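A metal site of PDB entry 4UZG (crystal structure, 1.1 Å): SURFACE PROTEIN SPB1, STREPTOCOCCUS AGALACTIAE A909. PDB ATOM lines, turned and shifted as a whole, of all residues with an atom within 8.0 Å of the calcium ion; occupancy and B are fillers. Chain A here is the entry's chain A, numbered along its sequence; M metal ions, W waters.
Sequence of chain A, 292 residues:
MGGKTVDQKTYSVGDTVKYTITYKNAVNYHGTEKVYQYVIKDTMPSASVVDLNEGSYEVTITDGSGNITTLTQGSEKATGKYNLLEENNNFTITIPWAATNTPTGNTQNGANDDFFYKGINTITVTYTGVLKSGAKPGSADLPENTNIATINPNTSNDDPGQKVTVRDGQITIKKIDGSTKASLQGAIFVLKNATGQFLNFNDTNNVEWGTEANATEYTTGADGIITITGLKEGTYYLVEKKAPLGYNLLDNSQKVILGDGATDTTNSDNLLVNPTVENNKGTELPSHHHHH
Within 4 Å of the calcium ion: Asn 206, Val 207 and Glu 208. Along chain A the residues within 4 Å of the calcium ion span positions 206 to 208. The nearest printed residue that does not touch the calcium ion is Asp 15 (4.5 Å).
O of Val 13 is in hydrogen-bond range of N of Val 207, at 2.9 Å. O of Glu 208 lies within hydrogen-bond range of N of Asn 200.
O of Val 207 binds the calcium ion, at 2.3 Å. Water W1 is bound to the calcium ion (2.4 Å). The calcium ion is bound by water W2. OD1 of Asn 206 binds the calcium ion. Water W3 binds the calcium ion. The calcium ion is bound by OE2 of Glu 208, 2.4 Å away. Water W4 binds the calcium ion, at 2.5 Å.
Water W1 bridges the side-chain carboxylate (OD1) of Asp 15 and the backbone carbonyl oxygen (O) of Val 13.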
ATOM      1  N   SER A  12     -12.107 -22.177 -18.110  1.00  0.00           N
ATOM      2  CA  SER A  12     -12.317 -23.609 -17.945  1.00  0.00           C
ATOM      3  C   SER A  12     -10.990 -24.286 -17.662  1.00  0.00           C
ATOM      4  O   SER A  12      -9.932 -23.863 -18.131  1.00  0.00           O
ATOM      5  CB  SER A  12     -12.922 -24.254 -19.199  1.00  0.00           C
ATOM      6  OG  SER A  12     -14.278 -23.879 -19.355  1.00  0.00           O
ATOM      7  N   VAL A  13     -11.050 -25.376 -16.882  1.00  0.00           N
ATOM      8  CA  VAL A  13      -9.902 -26.227 -16.674  1.00  0.00           C
ATOM      9  C   VAL A  13      -9.291 -26.613 -18.019  1.00  0.00           C
ATOM     10  O   VAL A  13     -10.010 -26.966 -18.964  1.00  0.00           O
ATOM     11  CB  VAL A  13     -10.309 -27.431 -15.809  1.00  0.00           C
ATOM     12  CG1 VAL A  13      -9.251 -28.528 -15.842  1.00  0.00           C
ATOM     13  CG2 VAL A  13     -10.569 -26.979 -14.375  1.00  0.00           C
ATOM     14  N   GLY A  14      -7.976 -26.488 -18.112  1.00  0.00           N
ATOM     15  CA  GLY A  14      -7.228 -26.702 -19.338  1.00  0.00           C
ATOM     16  C   GLY A  14      -6.912 -25.448 -20.146  1.00  0.00           C
ATOM     17  O   GLY A  14      -6.075 -25.503 -21.052  1.00  0.00           O
ATOM     18  N   ASP A  15      -7.573 -24.352 -19.822  1.00  0.00           N
ATOM     19  CA  ASP A  15      -7.353 -23.109 -20.555  1.00  0.00           C
ATOM     20  C   ASP A  15      -5.968 -22.518 -20.239  1.00  0.00           C
ATOM     21  O   ASP A  15      -5.403 -22.696 -19.155  1.00  0.00           O
ATOM     22  CB  ASP A  15      -8.383 -22.029 -20.188  1.00  0.00           C
ATOM     23  CG  ASP A  15      -9.763 -22.241 -20.784  1.00  0.00           C
ATOM     24  OD1 ASP A  15      -9.992 -23.188 -21.555  1.00  0.00           O
ATOM     25  OD2 ASP A  15     -10.619 -21.391 -20.443  1.00  0.00           O
ATOM     26  N   THR A  16      -5.456 -21.794 -21.212  1.00  0.00           N
ATOM     27  CA  THR A  16      -4.280 -20.950 -21.032  1.00  0.00           C
ATOM     28  C   THR A  16      -4.697 -19.660 -20.339  1.00  0.00           C
ATOM     29  O   THR A  16      -5.595 -18.945 -20.811  1.00  0.00           O
ATOM     30  CB  THR A  16      -3.644 -20.632 -22.382  1.00  0.00           C
ATOM     31  OG1 THR A  16      -3.264 -21.865 -22.990  1.00  0.00           O
ATOM     32  CG2 THR A  16      -2.414 -19.744 -22.215  1.00  0.00           C
ATOM     33  N   VAL A 130      -1.394 -22.868 -17.301  1.00  0.00           N
ATOM     34  CA  VAL A 130      -2.540 -23.685 -17.692  1.00  0.00           C
ATOM     35  C   VAL A 130      -3.325 -24.081 -16.452  1.00  0.00           C
ATOM     36  O   VAL A 130      -2.765 -24.615 -15.490  1.00  0.00           O
ATOM     37  CB  VAL A 130      -2.097 -24.931 -18.493  1.00  0.00           C
ATOM     38  CG1 VAL A 130      -3.284 -25.827 -18.811  1.00  0.00           C
ATOM     39  CG2 VAL A 130      -1.363 -24.525 -19.775  1.00  0.00           C
ATOM     40  N   ASN A 200     -16.356 -32.856 -23.443  1.00  0.00           N
ATOM     41  CA  ASN A 200     -15.541 -34.024 -23.167  1.00  0.00           C
ATOM     42  C   ASN A 200     -14.577 -33.607 -22.058  1.00  0.00           C
ATOM     43  O   ASN A 200     -13.735 -32.720 -22.258  1.00  0.00           O
ATOM     44  CB  ASN A 200     -14.770 -34.498 -24.391  1.00  0.00           C
ATOM     45  CG  ASN A 200     -13.855 -35.677 -24.035  1.00  0.00           C
ATOM     46  OD1 ASN A 200     -13.069 -35.639 -23.108  1.00  0.00           O
ATOM     47  ND2 ASN A 200     -14.040 -36.779 -24.726  1.00  0.00           N
ATOM     48  N   ASN A 205      -7.727 -32.809 -16.477  1.00  0.00           N
ATOM     49  CA  ASN A 205      -7.064 -31.505 -16.513  1.00  0.00           C
ATOM     50  C   ASN A 205      -7.395 -30.676 -17.751  1.00  0.00           C
ATOM     51  O   ASN A 205      -6.757 -29.636 -17.946  1.00  0.00           O
ATOM     52  CB  ASN A 205      -5.561 -31.669 -16.371  1.00  0.00           C
ATOM     53  CG  ASN A 205      -5.176 -32.193 -15.023  1.00  0.00           C
ATOM     54  OD1 ASN A 205      -5.480 -31.569 -13.995  1.00  0.00           O
ATOM     55  ND2 ASN A 205      -4.532 -33.370 -15.003  1.00  0.00           N
ATOM     56  N   ASN A 206      -8.378 -31.072 -18.564  1.00  0.00           N
ATOM     57  CA  ASN A 206      -8.641 -30.320 -19.766  1.00  0.00           C
ATOM     58  C   ASN A 206     -10.052 -30.489 -20.285  1.00  0.00           C
ATOM     59  O   ASN A 206     -10.381 -31.493 -20.931  1.00  0.00           O
ATOM     60  CB  ASN A 206      -7.636 -30.683 -20.864  1.00  0.00           C
ATOM     61  CG  ASN A 206      -7.826 -29.830 -22.092  1.00  0.00           C
ATOM     62  OD1 ASN A 206      -8.314 -28.698 -22.017  1.00  0.00           O
ATOM     63  ND2 ASN A 206      -7.400 -30.341 -23.216  1.00  0.00           N
ATOM     64  N   VAL A 207     -10.917 -29.495 -20.043  1.00  0.00           N
ATOM     65  CA  VAL A 207     -12.211 -29.398 -20.696  1.00  0.00           C
ATOM     66  C   VAL A 207     -12.021 -29.286 -22.193  1.00  0.00           C
ATOM     67  O   VAL A 207     -11.229 -28.453 -22.646  1.00  0.00           O
ATOM     68  CB  VAL A 207     -12.934 -28.123 -20.175  1.00  0.00           C
ATOM     69  CG1 VAL A 207     -14.094 -27.683 -21.072  1.00  0.00           C
ATOM     70  CG2 VAL A 207     -13.392 -28.294 -18.731  1.00  0.00           C
ATOM     71  N   GLU A 208     -12.770 -30.082 -22.965  1.00  0.00           N
ATOM     72  CA  GLU A 208     -12.762 -29.984 -24.409  1.00  0.00           C
ATOM     73  C   GLU A 208     -14.197 -29.963 -24.907  1.00  0.00           C
ATOM     74  O   GLU A 208     -15.119 -30.487 -24.260  1.00  0.00           O
ATOM     75  CB  GLU A 208     -12.010 -31.159 -25.023  1.00  0.00           C
ATOM     76  CG  GLU A 208     -10.476 -31.019 -24.896  1.00  0.00           C
ATOM     77  CD  GLU A 208      -9.929 -29.888 -25.778  1.00  0.00           C
ATOM     78  OE1 GLU A 208     -10.158 -29.907 -27.026  1.00  0.00           O
ATOM     79  OE2 GLU A 208      -9.387 -28.912 -25.262  1.00  0.00           O
ATOM     80  N   TRP A 209     -14.384 -29.356 -26.072  1.00  0.00           N
ATOM     81  CA  TRP A 209     -15.688 -29.175 -26.694  1.00  0.00           C
ATOM     82  C   TRP A 209     -15.646 -29.794 -28.080  1.00  0.00           C
ATOM     83  O   TRP A 209     -14.753 -29.488 -28.861  1.00  0.00           O
ATOM     84  CB  TRP A 209     -16.047 -27.695 -26.763  1.00  0.00           C
ATOM     85  CG  TRP A 209     -16.156 -27.062 -25.424  1.00  0.00           C
ATOM     86  CD1 TRP A 209     -15.237 -26.241 -24.833  1.00  0.00           C
ATOM     87  CD2 TRP A 209     -17.205 -27.255 -24.473  1.00  0.00           C
ATOM     88  NE1 TRP A 209     -15.645 -25.912 -23.575  1.00  0.00           N
ATOM     89  CE2 TRP A 209     -16.858 -26.507 -23.326  1.00  0.00           C
ATOM     90  CE3 TRP A 209     -18.420 -27.954 -24.488  1.00  0.00           C
ATOM     91  CZ2 TRP A 209     -17.672 -26.460 -22.203  1.00  0.00           C
ATOM     92  CZ3 TRP A 209     -19.217 -27.905 -23.393  1.00  0.00           C
ATOM     93  CH2 TRP A 209     -18.851 -27.167 -22.253  1.00  0.00           C
HETATM   94 CA    CA M   1      -9.451 -27.221 -23.529  1.00  0.00          CA
HETATM   95  O   HOH W   1      -9.813 -25.955 -21.576  1.00  0.00           O
HETATM   96  O   HOH W   2     -11.092 -26.361 -25.006  1.00  0.00           O
HETATM   97  O   HOH W   3      -7.180 -27.188 -24.328  1.00  0.00           O
HETATM   98  O   HOH W   4      -8.777 -24.834 -24.019  1.00  0.00           O
